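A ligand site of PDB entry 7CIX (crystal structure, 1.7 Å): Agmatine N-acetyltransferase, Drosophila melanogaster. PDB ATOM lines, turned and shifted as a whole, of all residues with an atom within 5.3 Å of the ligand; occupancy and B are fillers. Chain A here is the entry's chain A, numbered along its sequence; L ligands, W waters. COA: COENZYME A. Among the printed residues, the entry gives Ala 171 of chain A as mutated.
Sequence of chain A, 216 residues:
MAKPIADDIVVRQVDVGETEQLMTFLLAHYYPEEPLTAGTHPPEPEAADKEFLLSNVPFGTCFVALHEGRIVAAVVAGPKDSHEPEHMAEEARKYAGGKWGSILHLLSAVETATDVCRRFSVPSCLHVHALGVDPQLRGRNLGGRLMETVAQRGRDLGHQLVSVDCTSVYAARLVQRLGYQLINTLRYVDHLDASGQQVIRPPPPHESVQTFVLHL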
ATOM      1  N   HIS A  29       0.593  23.832  17.965  1.00  0.00           N
ATOM      2  CA  HIS A  29      -0.115  23.294  16.824  1.00  0.00           C
ATOM      3  C   HIS A  29       0.470  23.700  15.486  1.00  0.00           C
ATOM      4  O   HIS A  29      -0.010  23.223  14.457  1.00  0.00           O
ATOM      5  CB  HIS A  29      -1.587  23.696  16.884  1.00  0.00           C
ATOM      6  CG  HIS A  29      -2.306  23.106  18.051  1.00  0.00           C
ATOM      7  ND1 HIS A  29      -2.186  21.777  18.406  1.00  0.00           N
ATOM      8  CD2 HIS A  29      -3.150  23.655  18.958  1.00  0.00           C
ATOM      9  CE1 HIS A  29      -2.924  21.533  19.470  1.00  0.00           C
ATOM     10  NE2 HIS A  29      -3.528  22.659  19.825  1.00  0.00           N
ATOM     11  N   TYR A  30       1.484  24.561  15.466  1.00  0.00           N
ATOM     12  CA  TYR A  30       2.228  24.858  14.243  1.00  0.00           C
ATOM     13  C   TYR A  30       3.596  24.202  14.248  1.00  0.00           C
ATOM     14  O   TYR A  30       3.871  23.319  13.420  1.00  0.00           O
ATOM     15  CB  TYR A  30       2.382  26.388  14.064  1.00  0.00           C
ATOM     16  CG  TYR A  30       3.346  26.760  12.948  1.00  0.00           C
ATOM     17  CD1 TYR A  30       2.988  26.609  11.620  1.00  0.00           C
ATOM     18  CD2 TYR A  30       4.607  27.258  13.240  1.00  0.00           C
ATOM     19  CE1 TYR A  30       3.863  26.953  10.592  1.00  0.00           C
ATOM     20  CE2 TYR A  30       5.488  27.607  12.224  1.00  0.00           C
ATOM     21  CZ  TYR A  30       5.106  27.444  10.914  1.00  0.00           C
ATOM     22  OH  TYR A  30       5.999  27.783   9.913  1.00  0.00           O
ATOM     23  N   GLU A  33       4.525  20.127  14.069  1.00  0.00           N
ATOM     24  CA  GLU A  33       4.236  19.401  12.849  1.00  0.00           C
ATOM     25  C   GLU A  33       4.792  20.055  11.598  1.00  0.00           C
ATOM     26  O   GLU A  33       4.817  19.409  10.547  1.00  0.00           O
ATOM     27  CB  GLU A  33       2.720  19.223  12.678  1.00  0.00           C
ATOM     28  CG  GLU A  33       2.089  18.309  13.711  1.00  0.00           C
ATOM     29  CD  GLU A  33       0.587  18.378  13.675  1.00  0.00           C
ATOM     30  OE1 GLU A  33      -0.025  17.692  12.834  1.00  0.00           O
ATOM     31  OE2 GLU A  33       0.015  19.160  14.483  1.00  0.00           O
ATOM     32  N   GLU A  34       5.202  21.317  11.664  1.00  0.00           N
ATOM     33  CA  GLU A  34       5.721  21.978  10.481  1.00  0.00           C
ATOM     34  C   GLU A  34       6.982  21.248  10.013  1.00  0.00           C
ATOM     35  O   GLU A  34       7.895  21.015  10.814  1.00  0.00           O
ATOM     36  CB  GLU A  34       6.019  23.438  10.807  1.00  0.00           C
ATOM     37  CG  GLU A  34       6.277  24.297   9.573  1.00  0.00           C
ATOM     38  CD  GLU A  34       7.697  24.126   9.084  1.00  0.00           C
ATOM     39  OE1 GLU A  34       8.615  24.183   9.925  1.00  0.00           O
ATOM     40  OE2 GLU A  34       7.884  23.934   7.868  1.00  0.00           O
ATOM     41  N   PRO A  35       7.079  20.859   8.732  1.00  0.00           N
ATOM     42  CA  PRO A  35       8.142  19.930   8.325  1.00  0.00           C
ATOM     43  C   PRO A  35       9.565  20.448   8.521  1.00  0.00           C
ATOM     44  O   PRO A  35      10.443  19.657   8.877  1.00  0.00           O
ATOM     45  CB  PRO A  35       7.817  19.663   6.861  1.00  0.00           C
ATOM     46  CG  PRO A  35       6.335  19.789   6.788  1.00  0.00           C
ATOM     47  CD  PRO A  35       6.055  20.989   7.683  1.00  0.00           C
ATOM     48  N   ALA A 130       3.915  31.476   8.228  1.00  0.00           N
ATOM     49  CA  ALA A 130       3.440  30.376   9.050  1.00  0.00           C
ATOM     50  C   ALA A 130       1.931  30.281   8.914  1.00  0.00           C
ATOM     51  O   ALA A 130       1.248  31.301   8.780  1.00  0.00           O
ATOM     52  CB  ALA A 130       3.813  30.550  10.524  1.00  0.00           C
ATOM     53  N   LEU A 131       1.449  29.053   8.905  1.00  0.00           N
ATOM     54  CA  LEU A 131       0.029  28.775   8.862  1.00  0.00           C
ATOM     55  C   LEU A 131      -0.207  27.525   9.706  1.00  0.00           C
ATOM     56  O   LEU A 131       0.400  26.479   9.432  1.00  0.00           O
ATOM     57  CB  LEU A 131      -0.460  28.571   7.420  1.00  0.00           C
ATOM     58  CG  LEU A 131      -1.943  28.276   7.236  1.00  0.00           C
ATOM     59  CD1 LEU A 131      -2.833  29.468   7.625  1.00  0.00           C
ATOM     60  CD2 LEU A 131      -2.220  27.841   5.818  1.00  0.00           C
ATOM     61  N   GLY A 132      -1.055  27.636  10.729  1.00  0.00           N
ATOM     62  CA  GLY A 132      -1.343  26.494  11.575  1.00  0.00           C
ATOM     63  C   GLY A 132      -2.791  26.424  11.977  1.00  0.00           C
ATOM     64  O   GLY A 132      -3.416  27.454  12.217  1.00  0.00           O
ATOM     65  N   VAL A 133      -3.351  25.211  12.030  1.00  0.00           N
ATOM     66  CA  VAL A 133      -4.725  24.985  12.475  1.00  0.00           C
ATOM     67  C   VAL A 133      -4.690  23.936  13.584  1.00  0.00           C
ATOM     68  O   VAL A 133      -3.990  22.931  13.467  1.00  0.00           O
ATOM     69  CB  VAL A 133      -5.636  24.549  11.316  1.00  0.00           C
ATOM     70  CG1 VAL A 133      -7.035  24.172  11.822  1.00  0.00           C
ATOM     71  CG2 VAL A 133      -5.762  25.661  10.286  1.00  0.00           C
ATOM     72  N   LEU A 137      -9.710  21.062  14.563  1.00  0.00           N
ATOM     73  CA  LEU A 137     -10.501  21.894  13.655  1.00  0.00           C
ATOM     74  C   LEU A 137      -9.983  21.835  12.227  1.00  0.00           C
ATOM     75  O   LEU A 137     -10.356  22.668  11.401  1.00  0.00           O
ATOM     76  CB  LEU A 137     -10.547  23.340  14.153  1.00  0.00           C
ATOM     77  CG  LEU A 137     -11.530  23.611  15.301  1.00  0.00           C
ATOM     78  CD1 LEU A 137     -11.972  25.048  15.283  1.00  0.00           C
ATOM     79  CD2 LEU A 137     -12.745  22.699  15.208  1.00  0.00           C
ATOM     80  N   ARG A 138      -9.138  20.853  11.900  1.00  0.00           N
ATOM     81  CA  ARG A 138      -8.615  20.738  10.548  1.00  0.00           C
ATOM     82  C   ARG A 138      -9.678  20.164   9.614  1.00  0.00           C
ATOM     83  O   ARG A 138     -10.589  19.446  10.032  1.00  0.00           O
ATOM     84  CB  ARG A 138      -7.355  19.876  10.535  1.00  0.00           C
ATOM     85  CG  ARG A 138      -6.117  20.665  10.917  1.00  0.00           C
ATOM     86  CD  ARG A 138      -4.903  19.789  11.187  1.00  0.00           C
ATOM     87  NE  ARG A 138      -3.903  20.527  11.955  1.00  0.00           N
ATOM     88  CZ  ARG A 138      -2.797  20.002  12.444  1.00  0.00           C
ATOM     89  NH1 ARG A 138      -2.531  18.714  12.224  1.00  0.00           N
ATOM     90  NH2 ARG A 138      -1.934  20.743  13.127  1.00  0.00           N
ATOM     91  N   GLY A 139      -9.558  20.516   8.339  1.00  0.00           N
ATOM     92  CA  GLY A 139     -10.531  20.090   7.356  1.00  0.00           C
ATOM     93  C   GLY A 139     -11.800  20.913   7.332  1.00  0.00           C
ATOM     94  O   GLY A 139     -12.797  20.471   6.734  1.00  0.00           O
ATOM     95  N   ARG A 140     -11.793  22.085   7.959  1.00  0.00           N
ATOM     96  CA  ARG A 140     -12.988  22.916   8.074  1.00  0.00           C
ATOM     97  C   ARG A 140     -12.800  24.289   7.413  1.00  0.00           C
ATOM     98  O   ARG A 140     -13.487  25.246   7.780  1.00  0.00           O
ATOM     99  CB  ARG A 140     -13.395  23.064   9.540  1.00  0.00           C
ATOM    100  CG  ARG A 140     -14.479  22.062   9.968  1.00  0.00           C
ATOM    101  CD  ARG A 140     -14.472  21.791  11.476  1.00  0.00           C
ATOM    102  NE  ARG A 140     -13.499  20.771  11.838  1.00  0.00           N
ATOM    103  CZ  ARG A 140     -13.716  19.453  11.784  1.00  0.00           C
ATOM    104  NH1 ARG A 140     -12.755  18.607  12.139  1.00  0.00           N
ATOM    105  NH2 ARG A 140     -14.889  18.980  11.364  1.00  0.00           N
ATOM    106  N   ASN A 141     -11.863  24.403   6.470  1.00  0.00           N
ATOM    107  CA  ASN A 141     -11.586  25.620   5.707  1.00  0.00           C
ATOM    108  C   ASN A 141     -10.974  26.734   6.561  1.00  0.00           C
ATOM    109  O   ASN A 141     -11.005  27.897   6.160  1.00  0.00           O
ATOM    110  CB  ASN A 141     -12.851  26.146   5.006  1.00  0.00           C
ATOM    111  CG  ASN A 141     -12.527  27.036   3.809  1.00  0.00           C
ATOM    112  OD1 ASN A 141     -11.612  26.747   3.044  1.00  0.00           O
ATOM    113  ND2 ASN A 141     -13.277  28.123   3.669  1.00  0.00           N
ATOM    114  N   LEU A 142     -10.406  26.424   7.720  1.00  0.00           N
ATOM    115  CA  LEU A 142      -9.814  27.487   8.531  1.00  0.00           C
ATOM    116  C   LEU A 142      -8.522  27.994   7.907  1.00  0.00           C
ATOM    117  O   LEU A 142      -8.276  29.193   7.873  1.00  0.00           O
ATOM    118  CB  LEU A 142      -9.568  26.995   9.957  1.00  0.00           C
ATOM    119  CG  LEU A 142     -10.773  26.708  10.847  1.00  0.00           C
ATOM    120  CD1 LEU A 142     -10.343  26.554  12.300  1.00  0.00           C
ATOM    121  CD2 LEU A 142     -11.792  27.818  10.717  1.00  0.00           C
ATOM    122  N   GLY A 143      -7.677  27.080   7.418  1.00  0.00           N
ATOM    123  CA  GLY A 143      -6.492  27.517   6.693  1.00  0.00           C
ATOM    124  C   GLY A 143      -6.862  28.360   5.496  1.00  0.00           C
ATOM    125  O   GLY A 143      -6.300  29.436   5.275  1.00  0.00           O
ATOM    126  N   GLY A 144      -7.857  27.909   4.728  1.00  0.00           N
ATOM    127  CA  GLY A 144      -8.299  28.674   3.571  1.00  0.00           C
ATOM    128  C   GLY A 144      -8.796  30.062   3.944  1.00  0.00           C
ATOM    129  O   GLY A 144      -8.432  31.051   3.305  1.00  0.00           O
ATOM    130  N   VAL A 164       3.945  31.925  -0.736  1.00  0.00           N
ATOM    131  CA  VAL A 164       3.976  31.045   0.434  1.00  0.00           C
ATOM    132  C   VAL A 164       4.812  29.807   0.104  1.00  0.00           C
ATOM    133  O   VAL A 164       4.680  29.221  -0.980  1.00  0.00           O
ATOM    134  CB  VAL A 164       2.541  30.670   0.879  1.00  0.00           C
ATOM    135  CG1 VAL A 164       1.767  30.015  -0.282  1.00  0.00           C
ATOM    136  CG2 VAL A 164       2.573  29.737   2.090  1.00  0.00           C
ATOM    137  N   ASP A 165       5.674  29.420   1.048  1.00  0.00           N
ATOM    138  CA  ASP A 165       6.476  28.201   0.910  1.00  0.00           C
ATOM    139  C   ASP A 165       5.742  27.060   1.602  1.00  0.00           C
ATOM    140  O   ASP A 165       5.810  26.915   2.834  1.00  0.00           O
ATOM    141  CB  ASP A 165       7.858  28.381   1.524  1.00  0.00           C
ATOM    142  CG  ASP A 165       8.671  29.487   0.868  1.00  0.00           C
ATOM    143  OD1 ASP A 165       8.583  29.643  -0.367  1.00  0.00           O
ATOM    144  OD2 ASP A 165       9.421  30.191   1.594  1.00  0.00           O
ATOM    145  N   CYS A 166       5.047  26.231   0.820  1.00  0.00           N
ATOM    146  CA  CYS A 166       4.336  25.089   1.387  1.00  0.00           C
ATOM    147  C   CYS A 166       5.324  23.965   1.669  1.00  0.00           C
ATOM    148  O   CYS A 166       5.630  23.116   0.818  1.00  0.00           O
ATOM    149  CB  CYS A 166       3.203  24.667   0.460  1.00  0.00           C
ATOM    150  SG  CYS A 166       1.931  25.927   0.333  1.00  0.00           S
ATOM    151  N   THR A 167       5.890  24.002   2.881  1.00  0.00           N
ATOM    152  CA  THR A 167       6.770  22.945   3.354  1.00  0.00           C
ATOM    153  C   THR A 167       5.992  21.660   3.625  1.00  0.00           C
ATOM    154  O   THR A 167       6.593  20.581   3.640  1.00  0.00           O
ATOM    155  CB  THR A 167       7.466  23.402   4.634  1.00  0.00           C
ATOM    156  OG1 THR A 167       6.465  23.798   5.584  1.00  0.00           O
ATOM    157  CG2 THR A 167       8.357  24.615   4.346  1.00  0.00           C
ATOM    158  N   SER A 168       4.689  21.785   3.831  1.00  0.00           N
ATOM    159  CA  SER A 168       3.785  20.680   4.135  1.00  0.00           C
ATOM    160  C   SER A 168       2.944  20.360   2.909  1.00  0.00           C
ATOM    161  O   SER A 168       2.452  21.263   2.234  1.00  0.00           O
ATOM    162  CB  SER A 168       2.856  21.064   5.304  1.00  0.00           C
ATOM    163  OG  SER A 168       1.697  20.258   5.332  1.00  0.00           O
ATOM    164  N   TYR A 170      -0.001  19.196   3.021  1.00  0.00           N
ATOM    165  CA  TYR A 170      -1.368  19.632   3.295  1.00  0.00           C
ATOM    166  C   TYR A 170      -1.569  21.107   2.965  1.00  0.00           C
ATOM    167  O   TYR A 170      -2.645  21.511   2.509  1.00  0.00           O
ATOM    168  CB  TYR A 170      -1.711  19.349   4.759  1.00  0.00           C
ATOM    169  CG  TYR A 170      -1.455  17.914   5.127  1.00  0.00           C
ATOM    170  CD1 TYR A 170      -2.242  16.886   4.611  1.00  0.00           C
ATOM    171  CD2 TYR A 170      -0.402  17.572   5.975  1.00  0.00           C
ATOM    172  CE1 TYR A 170      -1.993  15.554   4.942  1.00  0.00           C
ATOM    173  CE2 TYR A 170      -0.140  16.245   6.305  1.00  0.00           C
ATOM    174  CZ  TYR A 170      -0.941  15.249   5.781  1.00  0.00           C
ATOM    175  OH  TYR A 170      -0.697  13.931   6.125  1.00  0.00           O
ATOM    176  N   ALA A 171      -0.539  21.930   3.173  1.00  0.00           N
ATOM    177  CA  ALA A 171      -0.626  23.328   2.803  1.00  0.00           C
ATOM    178  C   ALA A 171      -0.611  23.489   1.284  1.00  0.00           C
ATOM    179  O   ALA A 171      -1.329  24.328   0.743  1.00  0.00           O
ATOM    180  CB  ALA A 171       0.510  24.141   3.436  1.00  0.00           C
ATOM    181  N   LEU A 174      -3.991  22.837   0.044  1.00  0.00           N
ATOM    182  CA  LEU A 174      -4.901  23.922   0.373  1.00  0.00           C
ATOM    183  C   LEU A 174      -4.775  25.061  -0.621  1.00  0.00           C
ATOM    184  O   LEU A 174      -5.787  25.555  -1.163  1.00  0.00           O
ATOM    185  CB  LEU A 174      -4.604  24.418   1.794  1.00  0.00           C
ATOM    186  CG  LEU A 174      -5.077  25.834   2.133  1.00  0.00           C
ATOM    187  CD1 LEU A 174      -6.605  25.919   2.026  1.00  0.00           C
ATOM    188  CD2 LEU A 174      -4.640  26.233   3.544  1.00  0.00           C
ATOM    189  N   ARG A 177      -6.222  24.528  -4.134  1.00  0.00           N
ATOM    190  CA  ARG A 177      -7.652  24.733  -4.316  1.00  0.00           C
ATOM    191  C   ARG A 177      -8.071  26.182  -4.143  1.00  0.00           C
ATOM    192  O   ARG A 177      -9.147  26.559  -4.631  1.00  0.00           O
ATOM    193  CB  ARG A 177      -8.434  23.797  -3.393  1.00  0.00           C
ATOM    194  CG  ARG A 177      -8.548  24.230  -1.984  1.00  0.00           C
ATOM    195  CD  ARG A 177      -9.534  23.335  -1.241  1.00  0.00           C
ATOM    196  NE  ARG A 177      -9.516  23.619   0.195  1.00  0.00           N
ATOM    197  CZ  ARG A 177     -10.130  24.652   0.765  1.00  0.00           C
ATOM    198  NH1 ARG A 177     -10.817  25.516   0.013  1.00  0.00           N
ATOM    199  NH2 ARG A 177     -10.060  24.830   2.077  1.00  0.00           N
HETATM  200  N1A COA L   1      -2.400  16.018   8.751  1.00  0.00           N
HETATM  201  C2A COA L   1      -3.284  15.101   8.277  1.00  0.00           C
HETATM  202  N3A COA L   1      -4.414  15.526   7.613  1.00  0.00           N
HETATM  203  C4A COA L   1      -4.630  16.836   7.422  1.00  0.00           C
HETATM  204  C5A COA L   1      -3.747  17.740   7.895  1.00  0.00           C
HETATM  205  C6A COA L   1      -2.614  17.305   8.570  1.00  0.00           C
HETATM  206  N6A COA L   1      -1.377  17.865   9.254  1.00  0.00           N
HETATM  207  N7A COA L   1      -4.179  18.980   7.592  1.00  0.00           N
HETATM  208  C8A COA L   1      -5.349  18.890   6.918  1.00  0.00           C
HETATM  209  N9A COA L   1      -5.604  17.565   6.826  1.00  0.00           N
HETATM  210  C1B COA L   1      -6.594  16.839   6.291  1.00  0.00           C
HETATM  211  C2B COA L   1      -7.950  17.378   6.805  1.00  0.00           C
HETATM  212  O2B COA L   1      -8.406  16.724   8.064  1.00  0.00           O
HETATM  213  C3B COA L   1      -8.795  17.158   5.803  1.00  0.00           C
HETATM  214  O3B COA L   1      -9.209  15.764   5.786  1.00  0.00           O
HETATM  215  P3B COA L   1     -10.824  15.356   5.943  1.00  0.00           P
HETATM  216  O7A COA L   1     -11.292  15.681   7.348  1.00  0.00           O
HETATM  217  O8A COA L   1     -11.659  16.130   4.930  1.00  0.00           O
HETATM  218  O9A COA L   1     -10.970  13.871   5.670  1.00  0.00           O
HETATM  219  C4B COA L   1      -7.896  17.413   4.457  1.00  0.00           C
HETATM  220  O4B COA L   1      -6.640  17.145   4.761  1.00  0.00           O
HETATM  221  C5B COA L   1      -8.036  18.821   3.936  1.00  0.00           C
HETATM  222  O5B COA L   1      -8.079  19.739   5.024  1.00  0.00           O
HETATM  223  P1A COA L   1      -7.672  21.357   4.816  1.00  0.00           P
HETATM  224  O1A COA L   1      -7.123  21.615   3.411  1.00  0.00           O
HETATM  225  O2A COA L   1      -8.895  22.245   5.102  1.00  0.00           O
HETATM  226  O3A COA L   1      -6.463  21.656   5.917  1.00  0.00           O
HETATM  227  P2A COA L   1      -6.433  22.753   7.158  1.00  0.00           P
HETATM  228  O4A COA L   1      -7.447  22.455   8.221  1.00  0.00           O
HETATM  229  O5A COA L   1      -6.530  24.175   6.669  1.00  0.00           O
HETATM  230  O6A COA L   1      -4.914  22.486   7.740  1.00  0.00           O
HETATM  231  CBP COA L   1      -2.695  23.102   7.710  1.00  0.00           C
HETATM  232  CCP COA L   1      -3.890  22.749   6.854  1.00  0.00           C
HETATM  233  CDP COA L   1      -2.892  24.540   8.309  1.00  0.00           C
HETATM  234  CEP COA L   1      -1.419  23.055   6.855  1.00  0.00           C
HETATM  235  CAP COA L   1      -2.630  22.056   8.828  1.00  0.00           C
HETATM  236  OAP COA L   1      -2.265  20.812   8.281  1.00  0.00           O
HETATM  237  C9P COA L   1      -1.586  22.364   9.916  1.00  0.00           C
HETATM  238  O9P COA L   1      -1.778  23.161  10.775  1.00  0.00           O
HETATM  239  N8P COA L   1      -0.335  21.628   9.856  1.00  0.00           N
HETATM  240  C7P COA L   1       0.693  21.836  10.880  1.00  0.00           C
HETATM  241  C6P COA L   1       1.575  23.133  10.635  1.00  0.00           C
HETATM  242  C5P COA L   1       2.194  23.150   9.255  1.00  0.00           C
HETATM  243  O5P COA L   1       2.707  22.184   8.741  1.00  0.00           O
HETATM  244  N4P COA L   1       2.154  24.432   8.499  1.00  0.00           N
HETATM  245  C3P COA L   1       2.757  24.441   7.166  1.00  0.00           C
HETATM  246  C2P COA L   1       2.447  25.796   6.518  1.00  0.00           C
HETATM  247  S1P COA L   1       3.270  25.730   4.896  1.00  0.00           S
HETATM  248  O   HOH W   1      -9.773  23.886   8.780  1.00  0.00           O
HETATM  249  O   HOH W   2      -8.464  24.994   5.044  1.00  0.00           O
HETATM  250  O   HOH W   3      -0.578  14.267   9.890  1.00  0.00           O
HETATM  251  O   HOH W   4       1.463  20.029   8.059  1.00  0.00           O
HETATM  252  O   HOH W   5      -5.352  17.559   2.099  1.00  0.00           O
HETATM  253  O   HOH W   6     -13.008  13.364   3.788  1.00  0.00           O
HETATM  254  O   HOH W   7      -8.044  21.370   0.663  1.00  0.00           O
HETATM  255  O   HOH W   8      -5.101  20.200   2.615  1.00  0.00           O
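A nitrogen (N4P) of the ligand is in hydrogen-bond range of the backbone carbonyl oxygen (O) of Leu 131, 2.9 Å away. N of Gly 139 lies within hydrogen-bond range of O4A of the ligand (2.9 Å). The backbone NH (N) of Val 133 sits at hydrogen-bond distance from an oxygen (O9P) of the ligand (2.9 Å). NH2 of Arg 138 sits at hydrogen-bond distance from O9P of the ligand, at 3.4 Å. The backbone NH (N) of Gly 143 is in hydrogen-bond range of an oxygen (O5A) of the ligand. The backbone carbonyl oxygen (O) of Asp 165 lies close to a sulfur (S1P) of the ligand (3.5 Å). The backbone NH (N) of Thr 167 lies close to a sulfur (S1P) of the ligand (3.7 Å). The side-chain hydroxyl of Thr 167 sits close to a sulfur (S1P) of the ligand (3.8 Å).
The backbone carbonyl oxygen of Val 133 sits at hydrogen-bond distance from the guanidinium group of Arg 138. The side-chain carboxylate (OE1) of Glu 33 is in salt-bridge range of the guanidinium group (NH1) of Arg 138 (2.8 Å). The backbone carbonyl oxygen of His 29 sits at hydrogen-bond distance from the guanidinium group of Arg 138, 3.4 Å away. NH1 of Arg 140 is in hydrogen-bond range of O of Arg 138. The backbone NH (N) of Tyr 170 lies within hydrogen-bond range of the side-chain hydroxyl (OG) of Ser 168 (3.1 Å). The side-chain hydroxyl of Thr 167 lies within hydrogen-bond range of the side-chain carboxylate of Glu 34 (2.7 Å). The backbone carbonyl oxygen (O) of Ala 171 sits close to the side-chain sulfur (SG) of Cys 166, at 3.7 Å. OD1 of Asn 141 sits at hydrogen-bond distance from NH2 of Arg 177.
His 29 touches the ligand. O of Tyr 30 touches C6P of the ligand (3.6 Å). CB of Glu 33 touches C7P of the ligand, 3.8 Å away. Glu 34 touches the ligand (CA to O5P, 3.5 Å). CD of Pro 35 touches O5P of the ligand, at 3.7 Å. CA of Gly 132 touches O9P of the ligand, 3.5 Å away. Asn 141 touches the ligand (N to O2A, 3.9 Å). Cys 166 touches the ligand (CA to S1P, 3.7 Å). Ser 168 touches the ligand. Tyr 170 touches the ligand. CB of Ala 171 touches S1P of the ligand, at 3.5 Å. Hydrophobic or aromatic side chains that line the ligand: Tyr 30, Pro 35, Val 133, Tyr 170 and Ala 171. Within 4 Å of the ligand: His 29, Tyr 30, Glu 33, Glu 34, Pro 35, Leu 131, Gly 132, Val 133, Arg 138, Gly 139, Asn 141, Gly 143, Asp 165, Cys 166, Thr 167, Ser 168, Tyr 170 and Ala 171. The nearest printed residue that does not touch the ligand is Arg 140 (4.1 Å).
Water W4 bridges an oxygen (O5P) of the ligand (2.6 Å) and the side-chain hydroxyl (OG) of Ser 168 (2.7 Å). Water W8 bridges O1A of the ligand (2.6 Å) and O of Tyr 170 (2.8 Å). Water W7 lies within hydrogen-bond range of the guanidinium group of Arg 177 and an oxygen (O1A) of the ligand.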
